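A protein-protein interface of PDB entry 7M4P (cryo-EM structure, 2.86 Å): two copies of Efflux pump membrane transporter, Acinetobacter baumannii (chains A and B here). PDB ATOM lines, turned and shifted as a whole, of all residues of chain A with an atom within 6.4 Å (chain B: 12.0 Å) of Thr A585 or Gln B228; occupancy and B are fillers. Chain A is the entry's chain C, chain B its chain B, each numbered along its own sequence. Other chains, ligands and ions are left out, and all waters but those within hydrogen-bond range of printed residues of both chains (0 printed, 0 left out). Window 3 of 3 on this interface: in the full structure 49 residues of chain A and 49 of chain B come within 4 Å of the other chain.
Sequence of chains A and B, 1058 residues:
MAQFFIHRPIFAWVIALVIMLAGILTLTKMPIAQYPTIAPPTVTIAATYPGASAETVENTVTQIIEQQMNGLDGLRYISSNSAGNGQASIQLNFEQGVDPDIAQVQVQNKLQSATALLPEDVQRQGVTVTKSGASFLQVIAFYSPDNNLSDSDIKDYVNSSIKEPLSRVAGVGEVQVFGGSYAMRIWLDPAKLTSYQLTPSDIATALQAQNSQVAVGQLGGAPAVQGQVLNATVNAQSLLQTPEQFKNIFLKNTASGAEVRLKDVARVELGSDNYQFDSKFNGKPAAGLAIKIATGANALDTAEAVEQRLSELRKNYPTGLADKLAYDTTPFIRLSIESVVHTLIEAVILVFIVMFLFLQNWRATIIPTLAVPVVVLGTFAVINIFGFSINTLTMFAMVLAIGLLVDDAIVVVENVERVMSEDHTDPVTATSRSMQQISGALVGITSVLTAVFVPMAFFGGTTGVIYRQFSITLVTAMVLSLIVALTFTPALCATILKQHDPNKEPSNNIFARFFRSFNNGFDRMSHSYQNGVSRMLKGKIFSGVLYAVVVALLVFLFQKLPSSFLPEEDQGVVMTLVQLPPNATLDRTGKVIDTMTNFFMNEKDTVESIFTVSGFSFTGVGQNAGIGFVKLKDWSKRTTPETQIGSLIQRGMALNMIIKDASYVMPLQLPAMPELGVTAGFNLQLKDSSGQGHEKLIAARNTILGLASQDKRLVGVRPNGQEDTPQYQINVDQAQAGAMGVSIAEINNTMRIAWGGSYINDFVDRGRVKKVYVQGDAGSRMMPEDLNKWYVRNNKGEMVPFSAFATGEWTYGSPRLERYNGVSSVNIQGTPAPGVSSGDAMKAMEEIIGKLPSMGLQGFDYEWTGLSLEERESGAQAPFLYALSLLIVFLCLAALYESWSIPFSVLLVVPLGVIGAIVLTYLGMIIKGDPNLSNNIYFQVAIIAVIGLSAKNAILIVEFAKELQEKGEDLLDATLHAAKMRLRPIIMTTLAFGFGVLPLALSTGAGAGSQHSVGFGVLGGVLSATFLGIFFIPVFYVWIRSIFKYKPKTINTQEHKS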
ATOM      1  N   LEU A 580     -24.052  22.710 -11.722  1.00  0.00           N
ATOM      2  CA  LEU A 580     -23.389  21.492 -12.178  1.00  0.00           C
ATOM      3  C   LEU A 580     -22.119  21.879 -12.887  1.00  0.00           C
ATOM      4  O   LEU A 580     -21.968  23.004 -13.314  1.00  0.00           O
ATOM      5  CB  LEU A 580     -24.262  20.686 -13.137  1.00  0.00           C
ATOM      6  CG  LEU A 580     -24.879  19.357 -12.717  1.00  0.00           C
ATOM      7  CD1 LEU A 580     -26.236  19.577 -12.094  1.00  0.00           C
ATOM      8  CD2 LEU A 580     -25.003  18.448 -13.903  1.00  0.00           C
ATOM      9  N   PRO A 581     -21.192  20.942 -13.018  1.00  0.00           N
ATOM     10  CA  PRO A 581     -19.900  21.274 -13.609  1.00  0.00           C
ATOM     11  C   PRO A 581     -20.046  21.721 -15.050  1.00  0.00           C
ATOM     12  O   PRO A 581     -21.118  21.583 -15.650  1.00  0.00           O
ATOM     13  CB  PRO A 581     -19.120  19.961 -13.509  1.00  0.00           C
ATOM     14  CG  PRO A 581     -19.792  19.221 -12.428  1.00  0.00           C
ATOM     15  CD  PRO A 581     -21.216  19.568 -12.506  1.00  0.00           C
ATOM     16  N   ASN A 583     -20.093  21.999 -19.071  1.00  0.00           N
ATOM     17  CA  ASN A 583     -20.457  21.109 -20.168  1.00  0.00           C
ATOM     18  C   ASN A 583     -21.422  20.020 -19.743  1.00  0.00           C
ATOM     19  O   ASN A 583     -21.486  18.968 -20.375  1.00  0.00           O
ATOM     20  CB  ASN A 583     -19.220  20.477 -20.813  1.00  0.00           C
ATOM     21  CG  ASN A 583     -18.362  21.479 -21.546  1.00  0.00           C
ATOM     22  OD1 ASN A 583     -17.157  21.513 -21.361  1.00  0.00           O
ATOM     23  ND2 ASN A 583     -18.975  22.296 -22.376  1.00  0.00           N
ATOM     24  N   ALA A 584     -22.195  20.254 -18.693  1.00  0.00           N
ATOM     25  CA  ALA A 584     -23.142  19.268 -18.206  1.00  0.00           C
ATOM     26  C   ALA A 584     -24.486  19.444 -18.896  1.00  0.00           C
ATOM     27  O   ALA A 584     -24.959  20.563 -19.097  1.00  0.00           O
ATOM     28  CB  ALA A 584     -23.295  19.373 -16.691  1.00  0.00           C
ATOM     29  N   THR A 585     -25.098  18.325 -19.254  1.00  0.00           N
ATOM     30  CA  THR A 585     -26.275  18.315 -20.101  1.00  0.00           C
ATOM     31  C   THR A 585     -27.550  18.440 -19.269  1.00  0.00           C
ATOM     32  O   THR A 585     -27.523  18.457 -18.040  1.00  0.00           O
ATOM     33  CB  THR A 585     -26.284  17.041 -20.938  1.00  0.00           C
ATOM     34  OG1 THR A 585     -26.196  15.903 -20.080  1.00  0.00           O
ATOM     35  CG2 THR A 585     -25.126  17.035 -21.884  1.00  0.00           C
ATOM     36  N   LEU A 586     -28.688  18.534 -19.956  1.00  0.00           N
ATOM     37  CA  LEU A 586     -29.971  18.585 -19.267  1.00  0.00           C
ATOM     38  C   LEU A 586     -30.293  17.279 -18.570  1.00  0.00           C
ATOM     39  O   LEU A 586     -30.913  17.290 -17.507  1.00  0.00           O
ATOM     40  CB  LEU A 586     -31.092  18.919 -20.243  1.00  0.00           C
ATOM     41  CG  LEU A 586     -31.480  20.375 -20.438  1.00  0.00           C
ATOM     42  CD1 LEU A 586     -32.778  20.421 -21.191  1.00  0.00           C
ATOM     43  CD2 LEU A 586     -31.600  21.111 -19.116  1.00  0.00           C
ATOM     44  N   ASP A 587     -29.897  16.150 -19.146  1.00  0.00           N
ATOM     45  CA  ASP A 587     -30.166  14.870 -18.506  1.00  0.00           C
ATOM     46  C   ASP A 587     -29.487  14.776 -17.152  1.00  0.00           C
ATOM     47  O   ASP A 587     -30.099  14.352 -16.167  1.00  0.00           O
ATOM     48  CB  ASP A 587     -29.714  13.734 -19.411  1.00  0.00           C
ATOM     49  CG  ASP A 587     -30.678  13.487 -20.536  1.00  0.00           C
ATOM     50  OD1 ASP A 587     -31.533  14.364 -20.777  1.00  0.00           O
ATOM     51  OD2 ASP A 587     -30.597  12.414 -21.171  1.00  0.00           O
ATOM     52  N   ARG A 588     -28.225  15.185 -17.075  1.00  0.00           N
ATOM     53  CA  ARG A 588     -27.494  15.094 -15.817  1.00  0.00           C
ATOM     54  C   ARG A 588     -28.037  16.076 -14.789  1.00  0.00           C
ATOM     55  O   ARG A 588     -28.163  15.747 -13.602  1.00  0.00           O
ATOM     56  CB  ARG A 588     -26.011  15.332 -16.085  1.00  0.00           C
ATOM     57  CG  ARG A 588     -25.400  14.308 -17.017  1.00  0.00           C
ATOM     58  CD  ARG A 588     -24.131  14.824 -17.643  1.00  0.00           C
ATOM     59  NE  ARG A 588     -23.146  15.211 -16.647  1.00  0.00           N
ATOM     60  CZ  ARG A 588     -22.014  15.844 -16.915  1.00  0.00           C
ATOM     61  NH1 ARG A 588     -21.708  16.172 -18.158  1.00  0.00           N
ATOM     62  NH2 ARG A 588     -21.186  16.149 -15.935  1.00  0.00           N
ATOM     63  N   THR A 589     -28.386  17.280 -15.230  1.00  0.00           N
ATOM     64  CA  THR A 589     -28.995  18.243 -14.326  1.00  0.00           C
ATOM     65  C   THR A 589     -30.308  17.703 -13.772  1.00  0.00           C
ATOM     66  O   THR A 589     -30.569  17.789 -12.566  1.00  0.00           O
ATOM     67  CB  THR A 589     -29.197  19.569 -15.058  1.00  0.00           C
ATOM     68  OG1 THR A 589     -28.027  19.871 -15.818  1.00  0.00           O
ATOM     69  CG2 THR A 589     -29.431  20.702 -14.092  1.00  0.00           C
ATOM     70  N   GLY A 590     -31.121  17.094 -14.633  1.00  0.00           N
ATOM     71  CA  GLY A 590     -32.371  16.518 -14.180  1.00  0.00           C
ATOM     72  C   GLY A 590     -32.182  15.349 -13.235  1.00  0.00           C
ATOM     73  O   GLY A 590     -32.999  15.133 -12.345  1.00  0.00           O
ATOM     74  N   SER A 614     -35.505  22.316 -14.463  1.00  0.00           N
ATOM     75  CA  SER A 614     -34.146  22.027 -14.891  1.00  0.00           C
ATOM     76  C   SER A 614     -33.807  22.876 -16.103  1.00  0.00           C
ATOM     77  O   SER A 614     -34.612  23.006 -17.024  1.00  0.00           O
ATOM     78  CB  SER A 614     -33.972  20.550 -15.224  1.00  0.00           C
ATOM     79  OG  SER A 614     -32.629  20.159 -15.063  1.00  0.00           O
ATOM     80  N   GLN A 623     -27.851  24.610 -19.430  1.00  0.00           N
ATOM     81  CA  GLN A 623     -28.267  23.246 -19.169  1.00  0.00           C
ATOM     82  C   GLN A 623     -27.748  22.708 -17.841  1.00  0.00           C
ATOM     83  O   GLN A 623     -28.336  21.766 -17.306  1.00  0.00           O
ATOM     84  CB  GLN A 623     -27.827  22.354 -20.325  1.00  0.00           C
ATOM     85  CG  GLN A 623     -28.494  22.701 -21.632  1.00  0.00           C
ATOM     86  CD  GLN A 623     -28.408  21.586 -22.644  1.00  0.00           C
ATOM     87  OE1 GLN A 623     -28.091  20.450 -22.305  1.00  0.00           O
ATOM     88  NE2 GLN A 623     -28.698  21.902 -23.901  1.00  0.00           N
ATOM     89  N   ASN A 624     -26.696  23.294 -17.275  1.00  0.00           N
ATOM     90  CA  ASN A 624     -26.103  22.804 -16.038  1.00  0.00           C
ATOM     91  C   ASN A 624     -26.583  23.583 -14.819  1.00  0.00           C
ATOM     92  O   ASN A 624     -25.958  23.522 -13.761  1.00  0.00           O
ATOM     93  CB  ASN A 624     -24.579  22.835 -16.132  1.00  0.00           C
ATOM     94  CG  ASN A 624     -24.031  24.196 -16.512  1.00  0.00           C
ATOM     95  OD1 ASN A 624     -24.692  24.993 -17.172  1.00  0.00           O
ATOM     96  ND2 ASN A 624     -22.810  24.463 -16.099  1.00  0.00           N
ATOM     97  N   ARG A 781     -26.248  16.765 -34.989  1.00  0.00           N
ATOM     98  CA  ARG A 781     -25.776  18.006 -34.394  1.00  0.00           C
ATOM     99  C   ARG A 781     -25.315  17.826 -32.956  1.00  0.00           C
ATOM    100  O   ARG A 781     -25.418  18.764 -32.163  1.00  0.00           O
ATOM    101  CB  ARG A 781     -26.871  19.073 -34.490  1.00  0.00           C
ATOM    102  CG  ARG A 781     -28.253  18.609 -34.099  1.00  0.00           C
ATOM    103  CD  ARG A 781     -29.259  19.746 -34.128  1.00  0.00           C
ATOM    104  NE  ARG A 781     -30.574  19.301 -33.687  1.00  0.00           N
ATOM    105  CZ  ARG A 781     -30.988  19.293 -32.425  1.00  0.00           C
ATOM    106  NH1 ARG A 781     -32.199  18.857 -32.133  1.00  0.00           N
ATOM    107  NH2 ARG A 781     -30.200  19.714 -31.452  1.00  0.00           N
ATOM    108  N   MET A 782     -24.821  16.643 -32.596  1.00  0.00           N
ATOM    109  CA  MET A 782     -24.436  16.353 -31.222  1.00  0.00           C
ATOM    110  C   MET A 782     -22.951  16.533 -30.976  1.00  0.00           C
ATOM    111  O   MET A 782     -22.556  17.026 -29.919  1.00  0.00           O
ATOM    112  CB  MET A 782     -24.820  14.922 -30.858  1.00  0.00           C
ATOM    113  CG  MET A 782     -26.296  14.707 -30.648  1.00  0.00           C
ATOM    114  SD  MET A 782     -27.015  15.697 -29.336  1.00  0.00           S
ATOM    115  CE  MET A 782     -27.905  16.922 -30.267  1.00  0.00           C
ATOM    116  N   MET A 783     -22.130  16.157 -31.940  1.00  0.00           N
ATOM    117  CA  MET A 783     -20.691  16.017 -31.788  1.00  0.00           C
ATOM    118  C   MET A 783     -19.971  16.755 -32.896  1.00  0.00           C
ATOM    119  O   MET A 783     -20.531  16.982 -33.973  1.00  0.00           O
ATOM    120  CB  MET A 783     -20.326  14.531 -31.823  1.00  0.00           C
ATOM    121  CG  MET A 783     -21.018  13.715 -30.757  1.00  0.00           C
ATOM    122  SD  MET A 783     -20.639  14.276 -29.092  1.00  0.00           S
ATOM    123  CE  MET A 783     -18.860  14.222 -29.107  1.00  0.00           C
ATOM    124  N   GLY B 217     -24.264  27.472 -33.336  1.00  0.00           N
ATOM    125  CA  GLY B 217     -25.164  26.830 -32.396  1.00  0.00           C
ATOM    126  C   GLY B 217     -24.485  26.230 -31.184  1.00  0.00           C
ATOM    127  O   GLY B 217     -23.754  26.913 -30.463  1.00  0.00           O
ATOM    128  N   GLN B 218     -24.732  24.951 -30.936  1.00  0.00           N
ATOM    129  CA  GLN B 218     -24.240  24.297 -29.735  1.00  0.00           C
ATOM    130  C   GLN B 218     -24.019  22.819 -30.003  1.00  0.00           C
ATOM    131  O   GLN B 218     -24.670  22.226 -30.860  1.00  0.00           O
ATOM    132  CB  GLN B 218     -25.226  24.468 -28.583  1.00  0.00           C
ATOM    133  CG  GLN B 218     -24.791  25.448 -27.550  1.00  0.00           C
ATOM    134  CD  GLN B 218     -25.865  25.737 -26.561  1.00  0.00           C
ATOM    135  OE1 GLN B 218     -27.023  25.451 -26.799  1.00  0.00           O
ATOM    136  NE2 GLN B 218     -25.494  26.325 -25.439  1.00  0.00           N
ATOM    137  N   LEU B 219     -23.077  22.234 -29.271  1.00  0.00           N
ATOM    138  CA  LEU B 219     -22.959  20.786 -29.189  1.00  0.00           C
ATOM    139  C   LEU B 219     -23.964  20.272 -28.181  1.00  0.00           C
ATOM    140  O   LEU B 219     -24.175  20.891 -27.139  1.00  0.00           O
ATOM    141  CB  LEU B 219     -21.551  20.370 -28.768  1.00  0.00           C
ATOM    142  CG  LEU B 219     -20.411  20.826 -29.672  1.00  0.00           C
ATOM    143  CD1 LEU B 219     -19.098  20.349 -29.108  1.00  0.00           C
ATOM    144  CD2 LEU B 219     -20.597  20.335 -31.098  1.00  0.00           C
ATOM    145  N   GLY B 220     -24.602  19.151 -28.503  1.00  0.00           N
ATOM    146  CA  GLY B 220     -25.640  18.617 -27.648  1.00  0.00           C
ATOM    147  C   GLY B 220     -26.774  19.587 -27.414  1.00  0.00           C
ATOM    148  O   GLY B 220     -27.216  19.761 -26.280  1.00  0.00           O
ATOM    149  N   GLY B 221     -27.267  20.204 -28.480  1.00  0.00           N
ATOM    150  CA  GLY B 221     -28.299  21.213 -28.346  1.00  0.00           C
ATOM    151  C   GLY B 221     -29.588  20.652 -27.784  1.00  0.00           C
ATOM    152  O   GLY B 221     -29.838  19.452 -27.806  1.00  0.00           O
ATOM    153  N   ALA B 222     -30.440  21.564 -27.319  1.00  0.00           N
ATOM    154  CA  ALA B 222     -31.507  21.224 -26.380  1.00  0.00           C
ATOM    155  C   ALA B 222     -32.238  19.928 -26.696  1.00  0.00           C
ATOM    156  O   ALA B 222     -32.207  19.017 -25.853  1.00  0.00           O
ATOM    157  CB  ALA B 222     -32.493  22.394 -26.292  1.00  0.00           C
ATOM    158  N   PRO B 223     -32.891  19.749 -27.853  1.00  0.00           N
ATOM    159  CA  PRO B 223     -33.539  18.429 -28.004  1.00  0.00           C
ATOM    160  C   PRO B 223     -32.490  17.380 -28.359  1.00  0.00           C
ATOM    161  O   PRO B 223     -32.380  16.885 -29.469  1.00  0.00           O
ATOM    162  CB  PRO B 223     -34.561  18.670 -29.119  1.00  0.00           C
ATOM    163  CG  PRO B 223     -34.457  20.128 -29.474  1.00  0.00           C
ATOM    164  CD  PRO B 223     -33.124  20.594 -29.029  1.00  0.00           C
ATOM    165  N   ALA B 224     -31.691  17.023 -27.361  1.00  0.00           N
ATOM    166  CA  ALA B 224     -30.529  16.185 -27.584  1.00  0.00           C
ATOM    167  C   ALA B 224     -30.929  14.716 -27.669  1.00  0.00           C
ATOM    168  O   ALA B 224     -32.062  14.328 -27.397  1.00  0.00           O
ATOM    169  CB  ALA B 224     -29.492  16.395 -26.484  1.00  0.00           C
ATOM    170  N   VAL B 225     -29.971  13.908 -28.068  1.00  0.00           N
ATOM    171  CA  VAL B 225     -30.171  12.489 -28.279  1.00  0.00           C
ATOM    172  C   VAL B 225     -29.975  11.763 -26.955  1.00  0.00           C
ATOM    173  O   VAL B 225     -29.348  12.268 -26.026  1.00  0.00           O
ATOM    174  CB  VAL B 225     -29.210  11.970 -29.371  1.00  0.00           C
ATOM    175  CG1 VAL B 225     -27.779  11.995 -28.885  1.00  0.00           C
ATOM    176  CG2 VAL B 225     -29.594  10.578 -29.812  1.00  0.00           C
ATOM    177  N   GLN B 226     -30.538  10.567 -26.853  1.00  0.00           N
ATOM    178  CA  GLN B 226     -30.440   9.815 -25.611  1.00  0.00           C
ATOM    179  C   GLN B 226     -28.990   9.452 -25.337  1.00  0.00           C
ATOM    180  O   GLN B 226     -28.279   8.974 -26.222  1.00  0.00           O
ATOM    181  CB  GLN B 226     -31.298   8.555 -25.688  1.00  0.00           C
ATOM    182  CG  GLN B 226     -31.364   7.767 -24.393  1.00  0.00           C
ATOM    183  CD  GLN B 226     -32.032   8.545 -23.280  1.00  0.00           C
ATOM    184  OE1 GLN B 226     -32.757   9.507 -23.530  1.00  0.00           O
ATOM    185  NE2 GLN B 226     -31.787   8.135 -22.041  1.00  0.00           N
ATOM    186  N   GLY B 227     -28.550   9.681 -24.108  1.00  0.00           N
ATOM    187  CA  GLY B 227     -27.175   9.422 -23.752  1.00  0.00           C
ATOM    188  C   GLY B 227     -26.197  10.508 -24.118  1.00  0.00           C
ATOM    189  O   GLY B 227     -24.990  10.279 -24.027  1.00  0.00           O
ATOM    190  N   GLN B 228     -26.669  11.675 -24.534  1.00  0.00           N
ATOM    191  CA  GLN B 228     -25.767  12.775 -24.836  1.00  0.00           C
ATOM    192  C   GLN B 228     -24.971  13.140 -23.593  1.00  0.00           C
ATOM    193  O   GLN B 228     -25.515  13.231 -22.492  1.00  0.00           O
ATOM    194  CB  GLN B 228     -26.558  13.979 -25.350  1.00  0.00           C
ATOM    195  CG  GLN B 228     -25.741  15.227 -25.627  1.00  0.00           C
ATOM    196  CD  GLN B 228     -24.652  15.031 -26.660  1.00  0.00           C
ATOM    197  OE1 GLN B 228     -24.639  14.064 -27.402  1.00  0.00           O
ATOM    198  NE2 GLN B 228     -23.730  15.970 -26.713  1.00  0.00           N
ATOM    199  N   VAL B 229     -23.669  13.341 -23.772  1.00  0.00           N
ATOM    200  CA  VAL B 229     -22.767  13.480 -22.645  1.00  0.00           C
ATOM    201  C   VAL B 229     -22.217  14.893 -22.493  1.00  0.00           C
ATOM    202  O   VAL B 229     -21.866  15.284 -21.376  1.00  0.00           O
ATOM    203  CB  VAL B 229     -21.619  12.454 -22.746  1.00  0.00           C
ATOM    204  CG1 VAL B 229     -20.900  12.574 -24.077  1.00  0.00           C
ATOM    205  CG2 VAL B 229     -20.652  12.625 -21.595  1.00  0.00           C
ATOM    206  N   LEU B 230     -22.159  15.682 -23.562  1.00  0.00           N
ATOM    207  CA  LEU B 230     -21.522  16.988 -23.527  1.00  0.00           C
ATOM    208  C   LEU B 230     -22.421  18.054 -24.132  1.00  0.00           C
ATOM    209  O   LEU B 230     -23.165  17.802 -25.082  1.00  0.00           O
ATOM    210  CB  LEU B 230     -20.206  16.973 -24.287  1.00  0.00           C
ATOM    211  CG  LEU B 230     -19.239  18.047 -23.836  1.00  0.00           C
ATOM    212  CD1 LEU B 230     -18.488  17.542 -22.628  1.00  0.00           C
ATOM    213  CD2 LEU B 230     -18.299  18.416 -24.933  1.00  0.00           C
ATOM    214  N   ASN B 231     -22.333  19.258 -23.574  1.00  0.00           N
ATOM    215  CA  ASN B 231     -22.972  20.445 -24.125  1.00  0.00           C
ATOM    216  C   ASN B 231     -21.942  21.559 -24.152  1.00  0.00           C
ATOM    217  O   ASN B 231     -21.397  21.923 -23.107  1.00  0.00           O
ATOM    218  CB  ASN B 231     -24.189  20.851 -23.292  1.00  0.00           C
ATOM    219  CG  ASN B 231     -24.835  22.128 -23.781  1.00  0.00           C
ATOM    220  OD1 ASN B 231     -24.815  23.148 -23.103  1.00  0.00           O
ATOM    221  ND2 ASN B 231     -25.409  22.075 -24.961  1.00  0.00           N
ATOM    222  N   ALA B 232     -21.683  22.107 -25.336  1.00  0.00           N
ATOM    223  CA  ALA B 232     -20.736  23.194 -25.502  1.00  0.00           C
ATOM    224  C   ALA B 232     -21.239  24.139 -26.579  1.00  0.00           C
ATOM    225  O   ALA B 232     -22.110  23.796 -27.373  1.00  0.00           O
ATOM    226  CB  ALA B 232     -19.346  22.670 -25.866  1.00  0.00           C
ATOM    227  N   THR B 233     -20.681  25.341 -26.598  1.00  0.00           N
ATOM    228  CA  THR B 233     -21.022  26.358 -27.584  1.00  0.00           C
ATOM    229  C   THR B 233     -19.998  26.347 -28.707  1.00  0.00           C
ATOM    230  O   THR B 233     -18.795  26.294 -28.452  1.00  0.00           O
ATOM    231  CB  THR B 233     -21.070  27.739 -26.938  1.00  0.00           C
ATOM    232  OG1 THR B 233     -21.956  27.711 -25.821  1.00  0.00           O
ATOM    233  CG2 THR B 233     -21.557  28.772 -27.915  1.00  0.00           C
ATOM    234  N   VAL B 234     -20.475  26.385 -29.944  1.00  0.00           N
ATOM    235  CA  VAL B 234     -19.610  26.420 -31.115  1.00  0.00           C
ATOM    236  C   VAL B 234     -19.590  27.847 -31.632  1.00  0.00           C
ATOM    237  O   VAL B 234     -20.609  28.355 -32.106  1.00  0.00           O
ATOM    238  CB  VAL B 234     -20.082  25.450 -32.203  1.00  0.00           C
ATOM    239  CG1 VAL B 234     -18.963  25.225 -33.219  1.00  0.00           C
ATOM    240  CG2 VAL B 234     -20.552  24.140 -31.597  1.00  0.00           C
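The backbone carbonyl oxygen (O) of Met A782 sits at hydrogen-bond distance from the backbone NH (N) of Gly B220, 3.3 Å away.
O of Pro B223 is in hydrogen-bond range of NH1 of Arg A781 (3.3 Å).
The backbone NH of Val B225 sits at hydrogen-bond distance from the side-chain sulfur of Met A782.
OE1 of Gln B228 lies close to SD of Met A782 (3.5 Å).
The backbone carbonyl oxygen (O) of Val B229 is in hydrogen-bond range of the guanidinium group (NH1) of Arg A588 (3.3 Å).
The side-chain amide nitrogen of Asn A583 sits at hydrogen-bond distance from the backbone carbonyl oxygen of Asn B231, at 2.6 Å.
The side-chain amide nitrogen (ND2) of Asn B231 sits close to the side-chain amide nitrogen (NE2) of Gln A623, at 3.5 Å.
The side-chain amide nitrogen of Asn B231 lies within hydrogen-bond range of the backbone carbonyl oxygen of Leu B219, at 2.8 Å.
N of Leu B219 sits at hydrogen-bond distance from O of Ala B232 (2.6 Å).
The backbone carbonyl oxygen (O) of Gly B220 is in hydrogen-bond range of the side-chain amide nitrogen (ND2) of Asn B231.
The backbone carbonyl oxygen (O) of Thr A585 is in hydrogen-bond range of the side-chain hydroxyl (OG1) of Thr A589, at 2.7 Å.
The backbone NH of Leu A586 is in hydrogen-bond range of the side-chain amide oxygen of Gln A623 (3.1 Å).
O of Gln A623 sits at hydrogen-bond distance from OG1 of Thr A589, at 2.4 Å.
Among the printed residues, merely in contact across the chains: Gln A623 with Gly B220 (3.5 Å), Asn A583 with Leu B230 (3.5 Å), Asn A583 with Ala B232 (3.5 Å), Thr A585 with Leu B230 (3.7 Å), Thr A585 with Gln B228 (3.7 Å), Thr A585 with Val B229 (3.7 Å), Arg A781 with Gly B221 (3.7 Å), Met A782 with Leu B219 (3.7 Å), Arg A781 with Gly B220 (3.8 Å), Arg A781 with Gln B218 (3.8 Å), Met A782 with Gly B221 (3.8 Å), Gln A623 with Ala B222 (3.8 Å), Met A782 with Ala B224 (3.8 Å), Asn A583 with Val B229 (3.8 Å) and Thr A585 with Asn B231 (3.9 Å).
Of the printed residues of chain B, Thr A585 touches Gln B228, Val B229, Leu B230 and Asn B231.
No residue of chain B comes within 4 Å of Leu A586.
No residue of chain B comes within 4 Å of Asp A587.
Arg A588 touches just one residue of chain B: Val B229 (3.3 Å).
No residue of chain B comes within 4 Å of Thr A589.
Gln A623 touches just these residues of chain B: Gly B220 (3.5 Å), Ala B222 (3.8 Å) and Asn B231 (3.5 Å).
No residue of chain B comes within 4 Å of Asn A624.
Of the printed residues of chain A, Leu B219 touches Met A782.
Of the printed residues of chain A, Pro B223 touches Arg A781.
Of the printed residues of chain A, Asn B231 touches Asn A583, Thr A585 and Gln A623.
The nearest residue of chain B that does not touch Thr A585 is Gly B220 (5.6 Å).
The nearest printed residue of chain A that does not touch Gly B221 is Gln A623 (4.2 Å).
Of the 16 printed residues of chain A, 6 touch a printed residue of chain B.
Hydrophobic or aromatic side chains of chain A that line the printed part of chain B: Met A782.
Hydrophobic or aromatic side chains of chain B within 4 Å of the printed part of chain A: Leu B219, Pro B223, Ala B224, Val B225, Leu B230 and Ala B232.
Among the printed residues, no Asp or Glu carboxylate lies within 4 Å of a Lys or Arg side-chain nitrogen of the other chain.
No position is printed for both chains.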
